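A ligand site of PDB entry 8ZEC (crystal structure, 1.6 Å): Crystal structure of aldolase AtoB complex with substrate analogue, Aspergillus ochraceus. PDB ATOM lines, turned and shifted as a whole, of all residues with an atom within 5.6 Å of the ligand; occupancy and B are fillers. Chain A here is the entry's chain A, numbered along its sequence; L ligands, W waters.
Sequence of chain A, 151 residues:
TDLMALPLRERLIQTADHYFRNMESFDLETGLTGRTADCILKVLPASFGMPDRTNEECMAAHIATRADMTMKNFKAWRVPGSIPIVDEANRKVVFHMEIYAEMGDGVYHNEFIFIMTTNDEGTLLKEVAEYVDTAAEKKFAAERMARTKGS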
ATOM      1  N   TYR A  19       1.017  26.663  30.047  1.00  0.00           N
ATOM      2  CA  TYR A  19       0.769  27.085  28.663  1.00  0.00           C
ATOM      3  C   TYR A  19      -0.752  27.310  28.483  1.00  0.00           C
ATOM      4  O   TYR A  19      -1.205  28.251  27.832  1.00  0.00           O
ATOM      5  CB  TYR A  19       1.228  25.997  27.720  1.00  0.00           C
ATOM      6  CG  TYR A  19       1.034  26.254  26.239  1.00  0.00           C
ATOM      7  CD1 TYR A  19       1.963  26.937  25.492  1.00  0.00           C
ATOM      8  CD2 TYR A  19      -0.135  25.838  25.593  1.00  0.00           C
ATOM      9  CE1 TYR A  19       1.761  27.186  24.155  1.00  0.00           C
ATOM     10  CE2 TYR A  19      -0.351  26.045  24.243  1.00  0.00           C
ATOM     11  CZ  TYR A  19       0.596  26.745  23.524  1.00  0.00           C
ATOM     12  OH  TYR A  19       0.480  26.996  22.191  1.00  0.00           O
ATOM     13  N   ASN A  22      -2.192  30.193  30.731  1.00  0.00           N
ATOM     14  CA  ASN A  22      -1.834  31.421  30.037  1.00  0.00           C
ATOM     15  C   ASN A  22      -2.826  31.753  28.916  1.00  0.00           C
ATOM     16  O   ASN A  22      -3.237  32.920  28.784  1.00  0.00           O
ATOM     17  CB  ASN A  22      -0.392  31.335  29.583  1.00  0.00           C
ATOM     18  CG  ASN A  22       0.146  32.559  28.891  1.00  0.00           C
ATOM     19  OD1 ASN A  22       0.964  32.434  27.991  1.00  0.00           O
ATOM     20  ND2 ASN A  22      -0.179  33.742  29.394  1.00  0.00           N
ATOM     21  N   MET A  23      -3.154  30.752  28.065  1.00  0.00           N
ATOM     22  CA  MET A  23      -4.107  30.949  26.962  1.00  0.00           C
ATOM     23  C   MET A  23      -5.465  31.384  27.505  1.00  0.00           C
ATOM     24  O   MET A  23      -6.103  32.302  26.981  1.00  0.00           O
ATOM     25  CB  MET A  23      -4.260  29.661  26.168  1.00  0.00           C
ATOM     26  CG  MET A  23      -5.227  29.749  25.014  1.00  0.00           C
ATOM     27  SD  MET A  23      -5.375  28.126  24.225  1.00  0.00           S
ATOM     28  CE  MET A  23      -6.012  27.205  25.618  1.00  0.00           C
ATOM     29  N   PHE A  26      -5.216  35.095  28.855  1.00  0.00           N
ATOM     30  CA  PHE A  26      -4.408  35.900  27.955  1.00  0.00           C
ATOM     31  C   PHE A  26      -4.848  37.364  27.936  1.00  0.00           C
ATOM     32  O   PHE A  26      -6.039  37.630  27.766  1.00  0.00           O
ATOM     33  CB  PHE A  26      -4.579  35.304  26.552  1.00  0.00           C
ATOM     34  CG  PHE A  26      -3.806  36.006  25.466  1.00  0.00           C
ATOM     35  CD1 PHE A  26      -2.494  35.635  25.204  1.00  0.00           C
ATOM     36  CD2 PHE A  26      -4.392  36.979  24.668  1.00  0.00           C
ATOM     37  CE1 PHE A  26      -1.765  36.257  24.202  1.00  0.00           C
ATOM     38  CE2 PHE A  26      -3.660  37.588  23.669  1.00  0.00           C
ATOM     39  CZ  PHE A  26      -2.358  37.227  23.426  1.00  0.00           C
ATOM     40  N   LEU A  32       2.508  36.228  26.518  1.00  0.00           N
ATOM     41  CA  LEU A  32       2.810  34.799  26.685  1.00  0.00           C
ATOM     42  C   LEU A  32       3.878  34.678  27.769  1.00  0.00           C
ATOM     43  O   LEU A  32       4.885  35.410  27.752  1.00  0.00           O
ATOM     44  CB  LEU A  32       3.275  34.176  25.365  1.00  0.00           C
ATOM     45  CG  LEU A  32       2.307  34.348  24.194  1.00  0.00           C
ATOM     46  CD1 LEU A  32       2.870  33.891  22.877  1.00  0.00           C
ATOM     47  CD2 LEU A  32       1.017  33.644  24.456  1.00  0.00           C
ATOM     48  N   ARG A  35       7.737  30.926  29.177  1.00  0.00           N
ATOM     49  CA  ARG A  35       8.512  30.401  28.048  1.00  0.00           C
ATOM     50  C   ARG A  35       9.912  30.984  28.133  1.00  0.00           C
ATOM     51  O   ARG A  35      10.044  32.115  28.549  1.00  0.00           O
ATOM     52  CB  ARG A  35       7.818  30.776  26.730  1.00  0.00           C
ATOM     53  CG  ARG A  35       6.384  30.261  26.620  1.00  0.00           C
ATOM     54  CD  ARG A  35       5.974  30.365  25.157  1.00  0.00           C
ATOM     55  NE  ARG A  35       4.595  30.401  25.033  1.00  0.00           N
ATOM     56  CZ  ARG A  35       3.954  30.361  23.892  1.00  0.00           C
ATOM     57  NH1 ARG A  35       4.602  30.361  22.723  1.00  0.00           N
ATOM     58  NH2 ARG A  35       2.643  30.284  23.977  1.00  0.00           N
ATOM     59  N   LEU A  41       7.394  27.274  19.039  1.00  0.00           N
ATOM     60  CA  LEU A  41       6.159  26.557  18.766  1.00  0.00           C
ATOM     61  C   LEU A  41       6.258  25.854  17.420  1.00  0.00           C
ATOM     62  O   LEU A  41       6.320  26.506  16.375  1.00  0.00           O
ATOM     63  CB  LEU A  41       4.934  27.481  18.790  1.00  0.00           C
ATOM     64  CG  LEU A  41       3.604  26.781  18.436  1.00  0.00           C
ATOM     65  CD1 LEU A  41       3.155  25.814  19.512  1.00  0.00           C
ATOM     66  CD2 LEU A  41       2.499  27.792  18.134  1.00  0.00           C
ATOM     67  N   VAL A  43       4.190  23.293  14.811  1.00  0.00           N
ATOM     68  CA  VAL A  43       2.861  22.852  14.467  1.00  0.00           C
ATOM     69  C   VAL A  43       3.014  21.629  13.575  1.00  0.00           C
ATOM     70  O   VAL A  43       3.641  21.725  12.529  1.00  0.00           O
ATOM     71  CB  VAL A  43       1.987  23.930  13.827  1.00  0.00           C
ATOM     72  CG1 VAL A  43       0.675  23.336  13.372  1.00  0.00           C
ATOM     73  CG2 VAL A  43       1.737  25.047  14.796  1.00  0.00           C
ATOM     74  N   PHE A  48       0.642  20.362   7.160  1.00  0.00           N
ATOM     75  CA  PHE A  48      -0.257  21.482   7.449  1.00  0.00           C
ATOM     76  C   PHE A  48       0.382  22.796   6.989  1.00  0.00           C
ATOM     77  O   PHE A  48      -0.319  23.788   6.805  1.00  0.00           O
ATOM     78  CB  PHE A  48      -0.716  21.485   8.924  1.00  0.00           C
ATOM     79  CG  PHE A  48      -1.645  22.596   9.336  1.00  0.00           C
ATOM     80  CD1 PHE A  48      -2.976  22.589   8.998  1.00  0.00           C
ATOM     81  CD2 PHE A  48      -1.153  23.695  10.054  1.00  0.00           C
ATOM     82  CE1 PHE A  48      -3.797  23.670   9.310  1.00  0.00           C
ATOM     83  CE2 PHE A  48      -1.998  24.752  10.410  1.00  0.00           C
ATOM     84  CZ  PHE A  48      -3.313  24.741  10.043  1.00  0.00           C
ATOM     85  N   MET A  50       2.584  25.029   8.435  1.00  0.00           N
ATOM     86  CA  MET A  50       2.763  26.092   9.398  1.00  0.00           C
ATOM     87  C   MET A  50       4.203  26.040   9.846  1.00  0.00           C
ATOM     88  O   MET A  50       4.672  25.094  10.458  1.00  0.00           O
ATOM     89  CB  MET A  50       1.811  25.950  10.578  1.00  0.00           C
ATOM     90  CG  MET A  50       1.986  26.978  11.691  1.00  0.00           C
ATOM     91  SD  MET A  50       1.560  28.674  11.260  1.00  0.00           S
ATOM     92  CE  MET A  50      -0.231  28.563  11.182  1.00  0.00           C
ATOM     93  N   ARG A  53       7.531  28.926  15.013  1.00  0.00           N
ATOM     94  CA  ARG A  53       7.371  30.311  15.424  1.00  0.00           C
ATOM     95  C   ARG A  53       7.975  30.565  16.816  1.00  0.00           C
ATOM     96  O   ARG A  53       7.924  29.749  17.731  1.00  0.00           O
ATOM     97  CB  ARG A  53       5.902  30.702  15.428  1.00  0.00           C
ATOM     98  CG  ARG A  53       5.307  30.785  14.031  1.00  0.00           C
ATOM     99  CD  ARG A  53       3.817  31.091  14.102  1.00  0.00           C
ATOM    100  NE  ARG A  53       3.113  29.923  14.580  1.00  0.00           N
ATOM    101  CZ  ARG A  53       1.799  29.852  14.766  1.00  0.00           C
ATOM    102  NH1 ARG A  53       0.994  30.842  14.413  1.00  0.00           N
ATOM    103  NH2 ARG A  53       1.288  28.735  15.245  1.00  0.00           N
ATOM    104  N   HIS A  62      -1.787  35.329  17.657  1.00  0.00           N
ATOM    105  CA  HIS A  62      -2.918  35.133  18.562  1.00  0.00           C
ATOM    106  C   HIS A  62      -3.710  36.424  18.691  1.00  0.00           C
ATOM    107  O   HIS A  62      -4.909  36.401  18.761  1.00  0.00           O
ATOM    108  CB  HIS A  62      -2.510  34.625  19.951  1.00  0.00           C
ATOM    109  CG  HIS A  62      -1.779  33.343  19.919  1.00  0.00           C
ATOM    110  ND1 HIS A  62      -2.062  32.329  19.033  1.00  0.00           N
ATOM    111  CD2 HIS A  62      -0.722  32.892  20.660  1.00  0.00           C
ATOM    112  CE1 HIS A  62      -1.208  31.330  19.227  1.00  0.00           C
ATOM    113  NE2 HIS A  62      -0.407  31.640  20.221  1.00  0.00           N
ATOM    114  N   THR A  65      -5.764  36.607  15.436  1.00  0.00           N
ATOM    115  CA  THR A  65      -6.834  35.605  15.341  1.00  0.00           C
ATOM    116  C   THR A  65      -8.002  35.991  16.251  1.00  0.00           C
ATOM    117  O   THR A  65      -9.157  35.892  15.879  1.00  0.00           O
ATOM    118  CB  THR A  65      -6.302  34.199  15.659  1.00  0.00           C
ATOM    119  OG1 THR A  65      -5.222  33.901  14.757  1.00  0.00           O
ATOM    120  CG2 THR A  65      -7.386  33.170  15.486  1.00  0.00           C
ATOM    121  N   ARG A  66      -7.687  36.456  17.463  1.00  0.00           N
ATOM    122  CA  ARG A  66      -8.668  36.832  18.446  1.00  0.00           C
ATOM    123  C   ARG A  66      -9.454  38.034  17.970  1.00  0.00           C
ATOM    124  O   ARG A  66     -10.654  38.082  18.170  1.00  0.00           O
ATOM    125  CB  ARG A  66      -8.050  37.084  19.809  1.00  0.00           C
ATOM    126  CG  ARG A  66      -7.452  35.832  20.458  1.00  0.00           C
ATOM    127  CD  ARG A  66      -7.123  36.042  21.915  1.00  0.00           C
ATOM    128  NE  ARG A  66      -6.492  34.850  22.472  1.00  0.00           N
ATOM    129  CZ  ARG A  66      -6.710  34.360  23.691  1.00  0.00           C
ATOM    130  NH1 ARG A  66      -7.622  34.883  24.506  1.00  0.00           N
ATOM    131  NH2 ARG A  66      -6.054  33.285  24.083  1.00  0.00           N
ATOM    132  N   MET A  71     -12.668  36.147  19.115  1.00  0.00           N
ATOM    133  CA  MET A  71     -12.627  34.962  19.975  1.00  0.00           C
ATOM    134  C   MET A  71     -12.339  35.359  21.413  1.00  0.00           C
ATOM    135  O   MET A  71     -11.549  36.299  21.669  1.00  0.00           O
ATOM    136  CB  MET A  71     -11.512  34.012  19.541  1.00  0.00           C
ATOM    137  CG  MET A  71     -11.479  33.674  18.099  1.00  0.00           C
ATOM    138  SD  MET A  71     -10.262  32.452  17.572  1.00  0.00           S
ATOM    139  CE  MET A  71     -11.023  30.935  18.147  1.00  0.00           C
ATOM    140  N   PHE A  74     -11.538  31.352  26.234  1.00  0.00           N
ATOM    141  CA  PHE A  74     -10.770  30.164  25.951  1.00  0.00           C
ATOM    142  C   PHE A  74     -10.736  29.291  27.188  1.00  0.00           C
ATOM    143  O   PHE A  74     -10.647  29.778  28.321  1.00  0.00           O
ATOM    144  CB  PHE A  74      -9.345  30.476  25.519  1.00  0.00           C
ATOM    145  CG  PHE A  74      -9.200  30.949  24.106  1.00  0.00           C
ATOM    146  CD1 PHE A  74      -9.581  32.251  23.714  1.00  0.00           C
ATOM    147  CD2 PHE A  74      -8.751  30.073  23.131  1.00  0.00           C
ATOM    148  CE1 PHE A  74      -9.488  32.653  22.394  1.00  0.00           C
ATOM    149  CE2 PHE A  74      -8.611  30.491  21.810  1.00  0.00           C
ATOM    150  CZ  PHE A  74      -8.996  31.775  21.442  1.00  0.00           C
ATOM    151  N   ILE A  99      -9.294  22.202  23.140  1.00  0.00           N
ATOM    152  CA  ILE A  99      -9.317  23.648  23.301  1.00  0.00           C
ATOM    153  C   ILE A  99     -10.635  24.173  22.725  1.00  0.00           C
ATOM    154  O   ILE A  99     -10.993  23.850  21.595  1.00  0.00           O
ATOM    155  CB  ILE A  99      -8.119  24.312  22.613  1.00  0.00           C
ATOM    156  CG1 ILE A  99      -6.783  23.772  23.172  1.00  0.00           C
ATOM    157  CG2 ILE A  99      -8.239  25.858  22.739  1.00  0.00           C
ATOM    158  CD1 ILE A  99      -5.540  24.485  22.610  1.00  0.00           C
ATOM    159  N   TYR A 108     -15.176  27.486  18.579  1.00  0.00           N
ATOM    160  CA  TYR A 108     -13.996  26.765  18.165  1.00  0.00           C
ATOM    161  C   TYR A 108     -13.819  25.645  19.183  1.00  0.00           C
ATOM    162  O   TYR A 108     -13.729  25.931  20.367  1.00  0.00           O
ATOM    163  CB  TYR A 108     -12.803  27.732  18.122  1.00  0.00           C
ATOM    164  CG  TYR A 108     -11.442  27.061  17.891  1.00  0.00           C
ATOM    165  CD1 TYR A 108     -10.687  26.504  18.952  1.00  0.00           C
ATOM    166  CD2 TYR A 108     -10.862  27.044  16.630  1.00  0.00           C
ATOM    167  CE1 TYR A 108      -9.462  25.903  18.721  1.00  0.00           C
ATOM    168  CE2 TYR A 108      -9.617  26.454  16.398  1.00  0.00           C
ATOM    169  CZ  TYR A 108      -8.895  25.919  17.453  1.00  0.00           C
ATOM    170  OH  TYR A 108      -7.693  25.329  17.187  1.00  0.00           O
ATOM    171  N   PHE A 112      -6.207  17.817  20.189  1.00  0.00           N
ATOM    172  CA  PHE A 112      -4.796  18.070  19.941  1.00  0.00           C
ATOM    173  C   PHE A 112      -3.974  17.066  20.737  1.00  0.00           C
ATOM    174  O   PHE A 112      -4.474  16.597  21.783  1.00  0.00           O
ATOM    175  CB  PHE A 112      -4.324  19.449  20.470  1.00  0.00           C
ATOM    176  CG  PHE A 112      -5.028  20.619  19.842  1.00  0.00           C
ATOM    177  CD1 PHE A 112      -6.236  21.099  20.323  1.00  0.00           C
ATOM    178  CD2 PHE A 112      -4.459  21.216  18.754  1.00  0.00           C
ATOM    179  CE1 PHE A 112      -6.877  22.162  19.688  1.00  0.00           C
ATOM    180  CE2 PHE A 112      -5.068  22.299  18.148  1.00  0.00           C
ATOM    181  CZ  PHE A 112      -6.281  22.769  18.621  1.00  0.00           C
ATOM    182  N   PHE A 114      -0.360  17.793  22.581  1.00  0.00           N
ATOM    183  CA  PHE A 114       0.723  18.748  22.830  1.00  0.00           C
ATOM    184  C   PHE A 114       1.922  18.009  23.472  1.00  0.00           C
ATOM    185  O   PHE A 114       1.756  17.154  24.408  1.00  0.00           O
ATOM    186  CB  PHE A 114       0.284  19.796  23.843  1.00  0.00           C
ATOM    187  CG  PHE A 114      -0.599  20.911  23.317  1.00  0.00           C
ATOM    188  CD1 PHE A 114      -1.942  20.735  23.023  1.00  0.00           C
ATOM    189  CD2 PHE A 114       0.007  22.119  22.979  1.00  0.00           C
ATOM    190  CE1 PHE A 114      -2.689  21.774  22.469  1.00  0.00           C
ATOM    191  CE2 PHE A 114      -0.718  23.092  22.337  1.00  0.00           C
ATOM    192  CZ  PHE A 114      -2.066  22.971  22.133  1.00  0.00           C
ATOM    193  N   GLU A 130       2.566  21.014  18.797  1.00  0.00           N
ATOM    194  CA  GLU A 130       1.148  20.663  18.859  1.00  0.00           C
ATOM    195  C   GLU A 130       0.764  19.999  17.561  1.00  0.00           C
ATOM    196  O   GLU A 130       0.972  20.530  16.477  1.00  0.00           O
ATOM    197  CB  GLU A 130       0.257  21.890  19.159  1.00  0.00           C
ATOM    198  CG  GLU A 130       0.172  22.908  18.064  1.00  0.00           C
ATOM    199  CD  GLU A 130      -0.690  24.088  18.497  1.00  0.00           C
ATOM    200  OE1 GLU A 130      -1.847  23.877  18.964  1.00  0.00           O
ATOM    201  OE2 GLU A 130      -0.216  25.217  18.320  1.00  0.00           O
ATOM    202  N   VAL A 132      -2.226  18.973  15.352  1.00  0.00           N
ATOM    203  CA  VAL A 132      -3.563  19.515  15.190  1.00  0.00           C
ATOM    204  C   VAL A 132      -4.404  18.604  14.272  1.00  0.00           C
ATOM    205  O   VAL A 132      -3.889  17.776  13.506  1.00  0.00           O
ATOM    206  CB  VAL A 132      -3.481  20.940  14.596  1.00  0.00           C
ATOM    207  CG1 VAL A 132      -2.544  21.891  15.337  1.00  0.00           C
ATOM    208  CG2 VAL A 132      -3.108  20.855  13.153  1.00  0.00           C
ATOM    209  N   GLU A 137      -8.624  22.378  11.105  1.00  0.00           N
ATOM    210  CA  GLU A 137      -7.879  23.620  11.124  1.00  0.00           C
ATOM    211  C   GLU A 137      -7.892  24.245   9.734  1.00  0.00           C
ATOM    212  O   GLU A 137      -7.938  25.456   9.634  1.00  0.00           O
ATOM    213  CB  GLU A 137      -6.475  23.405  11.705  1.00  0.00           C
ATOM    214  CG  GLU A 137      -6.533  23.112  13.168  1.00  0.00           C
ATOM    215  CD  GLU A 137      -7.117  24.132  14.139  1.00  0.00           C
ATOM    216  OE1 GLU A 137      -7.366  25.306  13.759  1.00  0.00           O
ATOM    217  OE2 GLU A 137      -7.286  23.728  15.343  1.00  0.00           O
ATOM    218  N   PHE A 140     -11.094  26.092   9.629  1.00  0.00           N
ATOM    219  CA  PHE A 140     -11.093  27.314  10.418  1.00  0.00           C
ATOM    220  C   PHE A 140     -10.358  28.382   9.614  1.00  0.00           C
ATOM    221  O   PHE A 140     -10.836  29.516   9.525  1.00  0.00           O
ATOM    222  CB  PHE A 140     -10.553  27.061  11.825  1.00  0.00           C
ATOM    223  CG  PHE A 140     -10.364  28.305  12.661  1.00  0.00           C
ATOM    224  CD1 PHE A 140     -11.394  28.850  13.404  1.00  0.00           C
ATOM    225  CD2 PHE A 140      -9.150  28.968  12.658  1.00  0.00           C
ATOM    226  CE1 PHE A 140     -11.223  30.017  14.132  1.00  0.00           C
ATOM    227  CE2 PHE A 140      -8.981  30.146  13.373  1.00  0.00           C
ATOM    228  CZ  PHE A 140     -10.020  30.660  14.112  1.00  0.00           C
HETATM  229  C1  LIG L   1      -4.991  30.753  20.295  1.00  0.00           C
HETATM  230  C2  LIG L   1      -3.978  29.850  20.632  1.00  0.00           C
HETATM  231  C3  LIG L   1      -3.084  30.077  21.740  1.00  0.00           C
HETATM  232  C4  LIG L   1      -2.100  29.014  22.107  1.00  0.00           C
HETATM  233  C5  LIG L   1      -5.014  28.184  19.221  1.00  0.00           C
HETATM  234  C6  LIG L   1      -4.522  26.942  18.463  1.00  0.00           C
HETATM  235  C7  LIG L   1      -5.289  27.924  15.295  1.00  0.00           C
HETATM  236  C8  LIG L   1      -6.503  28.948  17.230  1.00  0.00           C
HETATM  237  C9  LIG L   1      -5.453  29.345  18.313  1.00  0.00           C
HETATM  238  C10 LIG L   1      -3.918  25.639  14.181  1.00  0.00           C
HETATM  239  C11 LIG L   1      -1.658  26.415  14.847  1.00  0.00           C
HETATM  240  C12 LIG L   1      -3.301  25.997  16.513  1.00  0.00           C
HETATM  241  C13 LIG L   1      -2.357  31.816  23.488  1.00  0.00           C
HETATM  242  C14 LIG L   1      -3.201  31.248  22.389  1.00  0.00           C
HETATM  243  O1  LIG L   1      -4.145  32.172  22.021  1.00  0.00           O
HETATM  244  C15 LIG L   1      -4.990  32.026  20.941  1.00  0.00           C
HETATM  245  O2  LIG L   1      -5.752  32.960  20.744  1.00  0.00           O
HETATM  246  O3  LIG L   1      -3.931  28.576  20.112  1.00  0.00           O
HETATM  247  C16 LIG L   1      -6.116  27.717  20.171  1.00  0.00           C
HETATM  248  O4  LIG L   1      -4.123  25.983  19.461  1.00  0.00           O
HETATM  249  C17 LIG L   1      -3.346  27.136  17.510  1.00  0.00           C
HETATM  250  O5  LIG L   1      -3.407  28.305  16.693  1.00  0.00           O
HETATM  251  C18 LIG L   1      -3.773  27.969  15.371  1.00  0.00           C
HETATM  252  O6  LIG L   1      -3.319  29.007  14.527  1.00  0.00           O
HETATM  253  C19 LIG L   1      -6.021  29.168  15.784  1.00  0.00           C
HETATM  254  C20 LIG L   1      -7.861  29.666  17.227  1.00  0.00           C
HETATM  255  C21 LIG L   1      -5.939  30.510  19.157  1.00  0.00           C
HETATM  256  C22 LIG L   1      -3.141  26.585  15.109  1.00  0.00           C
HETATM  257  O7  LIG L   1      -3.483  24.834  16.764  1.00  0.00           O
HETATM  258  O   HOH W   1      -1.845  31.041  14.144  1.00  0.00           O
HETATM  259  O   HOH W   2      -1.753  25.990  20.817  1.00  0.00           O
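The side-chain carboxylate (OE1) of Glu 130 lies within hydrogen-bond range of an oxygen (O4) of the ligand (3.1 Å). NE of Arg 66 sits at hydrogen-bond distance from O2 of the ligand, 2.7 Å away.
The side-chain carboxylate (OE2) of Glu 137 is in hydrogen-bond range of the side-chain hydroxyl (OH) of Tyr 108 (2.5 Å). The backbone carbonyl oxygen of Arg 53 lies within hydrogen-bond range of the backbone NH of Leu 41 (2.8 Å). O of Arg 66 is in hydrogen-bond range of N of Met 71 (2.9 Å). NH2 of Arg 66 is in hydrogen-bond range of O of Met 23.
Water W1 lies within hydrogen-bond range of an oxygen (O6) of the ligand (2.5 Å) and the guanidinium group (NH1) of Arg 53 (2.9 Å). Water W2 lies within hydrogen-bond range of O4 of the ligand (2.7 Å), OH of Tyr 19 (2.8 Å) and OE1 of Glu 130 (2.8 Å).
Tyr 19 touches the ligand (OH to C4, 3.3 Å). CG of Met 23 touches C14 of the ligand, 3.6 Å away. CD2 of Leu 32 touches C13 of the ligand (3.96 Å). CG2 of Val 43 touches C11 of the ligand, at 3.7 Å. NH2 of Arg 53 touches C11 of the ligand (3.8 Å). His 62 touches the ligand (CG to O1, 3.4 Å). CG2 of Thr 65 touches C20 of the ligand (3.9 Å). CE of Met 71 touches C20 of the ligand, 3.5 Å away. Phe 74 touches the ligand. Ile 99 touches the ligand (CD1 to O4, 3.8 Å). Tyr 108 touches the ligand. Phe 112 touches the ligand. Val 132 touches the ligand. Glu 137 touches the ligand. Phe 140 touches the ligand. Hydrophobic or aromatic side chains that line the ligand: Tyr 19, Met 23, Leu 32, Val 43, His 62, Met 71, Phe 74, Ile 99, Tyr 108, Phe 112, Val 132 and Phe 140. Within 4 Å of the ligand: Tyr 19, Met 23, Leu 32, Val 43, Arg 53, His 62, Thr 65, Arg 66, Met 71, Phe 74, Ile 99, Tyr 108, Phe 112, Glu 130, Val 132, Glu 137 and Phe 140.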
